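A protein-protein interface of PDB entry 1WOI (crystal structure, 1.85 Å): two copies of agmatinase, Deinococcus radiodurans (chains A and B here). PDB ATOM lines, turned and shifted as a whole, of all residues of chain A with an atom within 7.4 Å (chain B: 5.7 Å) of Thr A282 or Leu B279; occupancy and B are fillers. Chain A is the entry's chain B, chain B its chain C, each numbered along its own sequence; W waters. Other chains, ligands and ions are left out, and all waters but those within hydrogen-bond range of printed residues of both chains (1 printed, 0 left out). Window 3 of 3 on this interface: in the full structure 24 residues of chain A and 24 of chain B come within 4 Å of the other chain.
O of Thr A282 is in hydrogen-bond range of NH1 of Arg B45 (2.9 Å).
The backbone carbonyl oxygen (O) of Val A237 is in hydrogen-bond range of the guanidinium group (NE) of Arg A284 (3.4 Å). OD2 of Asp A280 lies within hydrogen-bond range of OG1 of Thr A282 (2.5 Å). The side-chain carboxylate (OD2) of Asp A280 lies within salt-bridge range of the guanidinium group (NH1) of Arg A284, at 3.8 Å. The guanidinium group (NH1) of Arg A284 sits at hydrogen-bond distance from the side-chain hydroxyl (OG1) of Thr A282, at 2.9 Å. O of Thr B241 lies within hydrogen-bond range of NH2 of Arg B45, 2.8 Å away. The side-chain hydroxyl (OG) of Ser B242 is in hydrogen-bond range of the backbone NH (N) of Arg B45, at 2.9 Å.
CG of Pro A281 touches CG of Pro B281, 3.5 Å away. CB of Thr A282 touches O of Leu B279 (3.3 Å). Arg A284 touches Pro B239 (NH1 to CB, 3.5 Å). CD1 of Leu A287 touches NH2 of Arg B45, 3.9 Å away.
Leu A279 touches none of the printed residues of chain B. Printed residues of chain B within 4 Å of Thr A282: Arg B45 and Leu B279. Of the printed residues of chain B, Arg A284 touches Pro B239. Of the printed residues of chain B, Leu A287 touches Arg B45. Of the printed residues of chain A, Arg B45 touches Thr A282 (2.9 Å) and Leu A287 (3.9 Å). Gly B240 touches none of the printed residues of chain A. Of chain A, only Thr A282 comes within 4 Å of Leu B279. The nearest residue of chain A that does not touch Leu B279 is Pro A281 (4.5 Å). The nearest printed residue of chain B that does not touch Pro A281 is Leu B279 (4.5 Å).
Of the 12 printed residues of chain A, 4 touch a printed residue of chain B. Printed residues of chain A that touch a printed residue of chain B: Pro A281, Thr A282, Arg A284 and Leu A287. Of the 12 printed residues of chain B, 4 touch a printed residue of chain A. Hydrophobic or aromatic side chains of chain B within 4 Å of the printed part of chain A: Pro B239 and Pro B281.
Pro B281 touches its own counterpart, Pro A281.
Water W1 lies within hydrogen-bond range of O of Thr A282 (2.8 Å), O of Pro B239 (2.8 Å) and NH2 of Arg B45 (3.0 Å).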
ATOM      1  N   VAL A 237       5.347 -12.148 -25.477  1.00  0.00           N
ATOM      2  CA  VAL A 237       5.047 -11.158 -24.453  1.00  0.00           C
ATOM      3  C   VAL A 237       4.449 -11.822 -23.216  1.00  0.00           C
ATOM      4  O   VAL A 237       4.903 -11.587 -22.095  1.00  0.00           O
ATOM      5  CB  VAL A 237       4.063 -10.088 -24.986  1.00  0.00           C
ATOM      6  CG1 VAL A 237       3.778  -9.042 -23.901  1.00  0.00           C
ATOM      7  CG2 VAL A 237       4.657  -9.418 -26.212  1.00  0.00           C
ATOM      8  N   PRO A 239       3.897 -15.547 -22.232  1.00  0.00           N
ATOM      9  CA  PRO A 239       4.001 -16.996 -22.436  1.00  0.00           C
ATOM     10  C   PRO A 239       3.223 -17.832 -21.428  1.00  0.00           C
ATOM     11  O   PRO A 239       2.927 -19.002 -21.682  1.00  0.00           O
ATOM     12  CB  PRO A 239       5.501 -17.244 -22.345  1.00  0.00           C
ATOM     13  CG  PRO A 239       5.918 -16.249 -21.291  1.00  0.00           C
ATOM     14  CD  PRO A 239       5.162 -14.996 -21.707  1.00  0.00           C
ATOM     15  N   PRO A 277       0.575 -18.739 -14.364  1.00  0.00           N
ATOM     16  CA  PRO A 277       1.836 -18.349 -13.724  1.00  0.00           C
ATOM     17  C   PRO A 277       2.893 -19.443 -13.737  1.00  0.00           C
ATOM     18  O   PRO A 277       4.082 -19.175 -13.926  1.00  0.00           O
ATOM     19  CB  PRO A 277       1.409 -17.983 -12.297  1.00  0.00           C
ATOM     20  CG  PRO A 277      -0.016 -17.597 -12.449  1.00  0.00           C
ATOM     21  CD  PRO A 277      -0.541 -18.618 -13.410  1.00  0.00           C
ATOM     22  N   LEU A 279       3.478 -21.483 -15.905  1.00  0.00           N
ATOM     23  CA  LEU A 279       4.063 -21.658 -17.230  1.00  0.00           C
ATOM     24  C   LEU A 279       5.036 -20.550 -17.638  1.00  0.00           C
ATOM     25  O   LEU A 279       5.610 -20.594 -18.727  1.00  0.00           O
ATOM     26  CB  LEU A 279       2.954 -21.805 -18.278  1.00  0.00           C
ATOM     27  CG  LEU A 279       2.072 -23.052 -18.134  1.00  0.00           C
ATOM     28  CD1 LEU A 279       1.049 -23.092 -19.266  1.00  0.00           C
ATOM     29  CD2 LEU A 279       2.933 -24.311 -18.168  1.00  0.00           C
ATOM     30  N   ASP A 280       5.225 -19.563 -16.766  1.00  0.00           N
ATOM     31  CA  ASP A 280       6.156 -18.475 -17.037  1.00  0.00           C
ATOM     32  C   ASP A 280       7.021 -18.214 -15.809  1.00  0.00           C
ATOM     33  O   ASP A 280       6.701 -17.360 -14.980  1.00  0.00           O
ATOM     34  CB  ASP A 280       5.421 -17.183 -17.407  1.00  0.00           C
ATOM     35  CG  ASP A 280       6.379 -16.052 -17.740  1.00  0.00           C
ATOM     36  OD1 ASP A 280       5.917 -14.915 -17.992  1.00  0.00           O
ATOM     37  OD2 ASP A 280       7.606 -16.305 -17.753  1.00  0.00           O
ATOM     38  N   PRO A 281       8.138 -18.947 -15.681  1.00  0.00           N
ATOM     39  CA  PRO A 281       9.038 -18.774 -14.536  1.00  0.00           C
ATOM     40  C   PRO A 281       9.724 -17.406 -14.473  1.00  0.00           C
ATOM     41  O   PRO A 281      10.357 -17.089 -13.474  1.00  0.00           O
ATOM     42  CB  PRO A 281      10.029 -19.924 -14.697  1.00  0.00           C
ATOM     43  CG  PRO A 281      10.094 -20.102 -16.181  1.00  0.00           C
ATOM     44  CD  PRO A 281       8.644 -19.982 -16.600  1.00  0.00           C
ATOM     45  N   THR A 282       9.611 -16.597 -15.528  1.00  0.00           N
ATOM     46  CA  THR A 282      10.230 -15.267 -15.503  1.00  0.00           C
ATOM     47  C   THR A 282       9.297 -14.305 -14.772  1.00  0.00           C
ATOM     48  O   THR A 282       9.694 -13.194 -14.414  1.00  0.00           O
ATOM     49  CB  THR A 282      10.453 -14.680 -16.910  1.00  0.00           C
ATOM     50  OG1 THR A 282       9.185 -14.329 -17.478  1.00  0.00           O
ATOM     51  CG2 THR A 282      11.169 -15.681 -17.820  1.00  0.00           C
ATOM     52  N   GLY A 283       8.054 -14.741 -14.581  1.00  0.00           N
ATOM     53  CA  GLY A 283       7.051 -13.938 -13.900  1.00  0.00           C
ATOM     54  C   GLY A 283       6.550 -12.709 -14.645  1.00  0.00           C
ATOM     55  O   GLY A 283       5.751 -11.944 -14.095  1.00  0.00           O
ATOM     56  N   ARG A 284       6.993 -12.503 -15.886  1.00  0.00           N
ATOM     57  CA  ARG A 284       6.553 -11.321 -16.638  1.00  0.00           C
ATOM     58  C   ARG A 284       5.087 -11.359 -17.058  1.00  0.00           C
ATOM     59  O   ARG A 284       4.461 -10.312 -17.225  1.00  0.00           O
ATOM     60  CB  ARG A 284       7.431 -11.082 -17.883  1.00  0.00           C
ATOM     61  CG  ARG A 284       7.243 -12.040 -19.062  1.00  0.00           C
ATOM     62  CD  ARG A 284       8.079 -11.539 -20.241  1.00  0.00           C
ATOM     63  NE  ARG A 284       8.093 -12.419 -21.411  1.00  0.00           N
ATOM     64  CZ  ARG A 284       8.683 -13.613 -21.453  1.00  0.00           C
ATOM     65  NH1 ARG A 284       9.312 -14.096 -20.384  1.00  0.00           N
ATOM     66  NH2 ARG A 284       8.668 -14.314 -22.580  1.00  0.00           N
ATOM     67  N   SER A 285       4.534 -12.554 -17.216  1.00  0.00           N
ATOM     68  CA  SER A 285       3.138 -12.676 -17.621  1.00  0.00           C
ATOM     69  C   SER A 285       2.201 -12.041 -16.590  1.00  0.00           C
ATOM     70  O   SER A 285       1.398 -11.174 -16.932  1.00  0.00           O
ATOM     71  CB  SER A 285       2.779 -14.145 -17.840  1.00  0.00           C
ATOM     72  OG  SER A 285       3.506 -14.680 -18.936  1.00  0.00           O
ATOM     73  N   GLU A 286       2.305 -12.452 -15.330  1.00  0.00           N
ATOM     74  CA  GLU A 286       1.434 -11.878 -14.307  1.00  0.00           C
ATOM     75  C   GLU A 286       1.718 -10.387 -14.086  1.00  0.00           C
ATOM     76  O   GLU A 286       0.796  -9.593 -13.908  1.00  0.00           O
ATOM     77  CB  GLU A 286       1.567 -12.641 -12.984  1.00  0.00           C
ATOM     78  CG  GLU A 286       2.994 -12.841 -12.497  1.00  0.00           C
ATOM     79  CD  GLU A 286       3.528 -14.222 -12.832  1.00  0.00           C
ATOM     80  OE1 GLU A 286       3.775 -14.999 -11.886  1.00  0.00           O
ATOM     81  OE2 GLU A 286       3.694 -14.536 -14.036  1.00  0.00           O
ATOM     82  N   LEU A 287       2.988  -9.999 -14.106  1.00  0.00           N
ATOM     83  CA  LEU A 287       3.325  -8.590 -13.907  1.00  0.00           C
ATOM     84  C   LEU A 287       2.692  -7.699 -14.977  1.00  0.00           C
ATOM     85  O   LEU A 287       2.102  -6.660 -14.670  1.00  0.00           O
ATOM     86  CB  LEU A 287       4.845  -8.391 -13.910  1.00  0.00           C
ATOM     87  CG  LEU A 287       5.601  -8.909 -12.681  1.00  0.00           C
ATOM     88  CD1 LEU A 287       7.095  -8.667 -12.848  1.00  0.00           C
ATOM     89  CD2 LEU A 287       5.094  -8.194 -11.436  1.00  0.00           C
ATOM     90  N   ARG B  45      12.731  -7.860  -6.940  1.00  0.00           N
ATOM     91  CA  ARG B  45      13.345  -9.179  -7.083  1.00  0.00           C
ATOM     92  C   ARG B  45      14.870  -9.185  -7.212  1.00  0.00           C
ATOM     93  O   ARG B  45      15.425  -8.699  -8.195  1.00  0.00           O
ATOM     94  CB  ARG B  45      12.722  -9.891  -8.289  1.00  0.00           C
ATOM     95  CG  ARG B  45      11.212 -10.067  -8.177  1.00  0.00           C
ATOM     96  CD  ARG B  45      10.658 -10.847  -9.354  1.00  0.00           C
ATOM     97  NE  ARG B  45      10.860 -10.147 -10.617  1.00  0.00           N
ATOM     98  CZ  ARG B  45      10.535 -10.650 -11.805  1.00  0.00           C
ATOM     99  NH1 ARG B  45       9.992 -11.857 -11.884  1.00  0.00           N
ATOM    100  NH2 ARG B  45      10.753  -9.947 -12.909  1.00  0.00           N
ATOM    101  N   PRO B  46      15.567  -9.764  -6.220  1.00  0.00           N
ATOM    102  CA  PRO B  46      17.034  -9.864  -6.173  1.00  0.00           C
ATOM    103  C   PRO B  46      17.580 -10.815  -7.236  1.00  0.00           C
ATOM    104  O   PRO B  46      16.837 -11.616  -7.800  1.00  0.00           O
ATOM    105  CB  PRO B  46      17.308 -10.421  -4.772  1.00  0.00           C
ATOM    106  CG  PRO B  46      16.058 -10.147  -4.010  1.00  0.00           C
ATOM    107  CD  PRO B  46      14.972 -10.363  -5.018  1.00  0.00           C
ATOM    108  N   PRO B 239      13.830 -10.800 -20.428  1.00  0.00           N
ATOM    109  CA  PRO B 239      12.961 -10.957 -19.254  1.00  0.00           C
ATOM    110  C   PRO B 239      13.687 -11.061 -17.921  1.00  0.00           C
ATOM    111  O   PRO B 239      13.073 -10.910 -16.865  1.00  0.00           O
ATOM    112  CB  PRO B 239      12.182 -12.227 -19.577  1.00  0.00           C
ATOM    113  CG  PRO B 239      13.217 -13.048 -20.281  1.00  0.00           C
ATOM    114  CD  PRO B 239      13.874 -12.044 -21.217  1.00  0.00           C
ATOM    115  N   GLY B 240      14.988 -11.324 -17.974  1.00  0.00           N
ATOM    116  CA  GLY B 240      15.763 -11.467 -16.755  1.00  0.00           C
ATOM    117  C   GLY B 240      16.078 -10.146 -16.079  1.00  0.00           C
ATOM    118  O   GLY B 240      17.195  -9.631 -16.193  1.00  0.00           O
ATOM    119  N   THR B 241      15.091  -9.589 -15.386  1.00  0.00           N
ATOM    120  CA  THR B 241      15.298  -8.327 -14.683  1.00  0.00           C
ATOM    121  C   THR B 241      14.213  -8.155 -13.616  1.00  0.00           C
ATOM    122  O   THR B 241      13.097  -8.663 -13.751  1.00  0.00           O
ATOM    123  CB  THR B 241      15.313  -7.136 -15.673  1.00  0.00           C
ATOM    124  OG1 THR B 241      15.866  -5.985 -15.025  1.00  0.00           O
ATOM    125  CG2 THR B 241      13.912  -6.806 -16.153  1.00  0.00           C
ATOM    126  N   SER B 242      14.547  -7.440 -12.549  1.00  0.00           N
ATOM    127  CA  SER B 242      13.621  -7.250 -11.437  1.00  0.00           C
ATOM    128  C   SER B 242      12.254  -6.647 -11.746  1.00  0.00           C
ATOM    129  O   SER B 242      11.220  -7.210 -11.374  1.00  0.00           O
ATOM    130  CB  SER B 242      14.286  -6.398 -10.349  1.00  0.00           C
ATOM    131  OG  SER B 242      13.393  -6.185  -9.261  1.00  0.00           O
ATOM    132  N   ALA B 276      19.212  -9.947 -14.220  1.00  0.00           N
ATOM    133  CA  ALA B 276      18.880 -10.919 -13.180  1.00  0.00           C
ATOM    134  C   ALA B 276      18.802 -12.282 -13.858  1.00  0.00           C
ATOM    135  O   ALA B 276      17.724 -12.710 -14.279  1.00  0.00           O
ATOM    136  CB  ALA B 276      17.542 -10.565 -12.553  1.00  0.00           C
ATOM    137  N   PRO B 277      19.948 -12.980 -13.969  1.00  0.00           N
ATOM    138  CA  PRO B 277      20.076 -14.300 -14.602  1.00  0.00           C
ATOM    139  C   PRO B 277      19.093 -15.316 -14.047  1.00  0.00           C
ATOM    140  O   PRO B 277      18.551 -16.144 -14.783  1.00  0.00           O
ATOM    141  CB  PRO B 277      21.520 -14.711 -14.292  1.00  0.00           C
ATOM    142  CG  PRO B 277      22.209 -13.432 -13.942  1.00  0.00           C
ATOM    143  CD  PRO B 277      21.171 -12.646 -13.217  1.00  0.00           C
ATOM    144  N   ASN B 278      18.886 -15.250 -12.738  1.00  0.00           N
ATOM    145  CA  ASN B 278      17.984 -16.158 -12.046  1.00  0.00           C
ATOM    146  C   ASN B 278      16.527 -16.011 -12.499  1.00  0.00           C
ATOM    147  O   ASN B 278      15.716 -16.913 -12.291  1.00  0.00           O
ATOM    148  CB  ASN B 278      18.095 -15.925 -10.533  1.00  0.00           C
ATOM    149  CG  ASN B 278      17.809 -14.481 -10.139  1.00  0.00           C
ATOM    150  OD1 ASN B 278      18.337 -13.544 -10.742  1.00  0.00           O
ATOM    151  ND2 ASN B 278      16.981 -14.299  -9.116  1.00  0.00           N
ATOM    152  N   LEU B 279      16.198 -14.887 -13.132  1.00  0.00           N
ATOM    153  CA  LEU B 279      14.827 -14.655 -13.588  1.00  0.00           C
ATOM    154  C   LEU B 279      14.592 -15.004 -15.064  1.00  0.00           C
ATOM    155  O   LEU B 279      13.517 -14.737 -15.612  1.00  0.00           O
ATOM    156  CB  LEU B 279      14.421 -13.202 -13.311  1.00  0.00           C
ATOM    157  CG  LEU B 279      14.495 -12.785 -11.831  1.00  0.00           C
ATOM    158  CD1 LEU B 279      14.146 -11.305 -11.673  1.00  0.00           C
ATOM    159  CD2 LEU B 279      13.533 -13.630 -11.013  1.00  0.00           C
ATOM    160  N   ASP B 280      15.594 -15.598 -15.707  1.00  0.00           N
ATOM    161  CA  ASP B 280      15.463 -16.022 -17.100  1.00  0.00           C
ATOM    162  C   ASP B 280      16.111 -17.386 -17.278  1.00  0.00           C
ATOM    163  O   ASP B 280      17.291 -17.481 -17.605  1.00  0.00           O
ATOM    164  CB  ASP B 280      16.126 -15.043 -18.067  1.00  0.00           C
ATOM    165  CG  ASP B 280      15.976 -15.480 -19.523  1.00  0.00           C
ATOM    166  OD1 ASP B 280      16.475 -14.775 -20.420  1.00  0.00           O
ATOM    167  OD2 ASP B 280      15.347 -16.534 -19.776  1.00  0.00           O
ATOM    168  N   PRO B 281      15.342 -18.463 -17.072  1.00  0.00           N
ATOM    169  CA  PRO B 281      15.903 -19.808 -17.226  1.00  0.00           C
ATOM    170  C   PRO B 281      16.291 -20.197 -18.653  1.00  0.00           C
ATOM    171  O   PRO B 281      16.913 -21.231 -18.856  1.00  0.00           O
ATOM    172  CB  PRO B 281      14.817 -20.706 -16.637  1.00  0.00           C
ATOM    173  CG  PRO B 281      13.557 -19.944 -16.926  1.00  0.00           C
ATOM    174  CD  PRO B 281      13.956 -18.521 -16.581  1.00  0.00           C
HETATM  175  O   HOH W   1      10.477 -10.880 -15.700  1.00  0.00           O
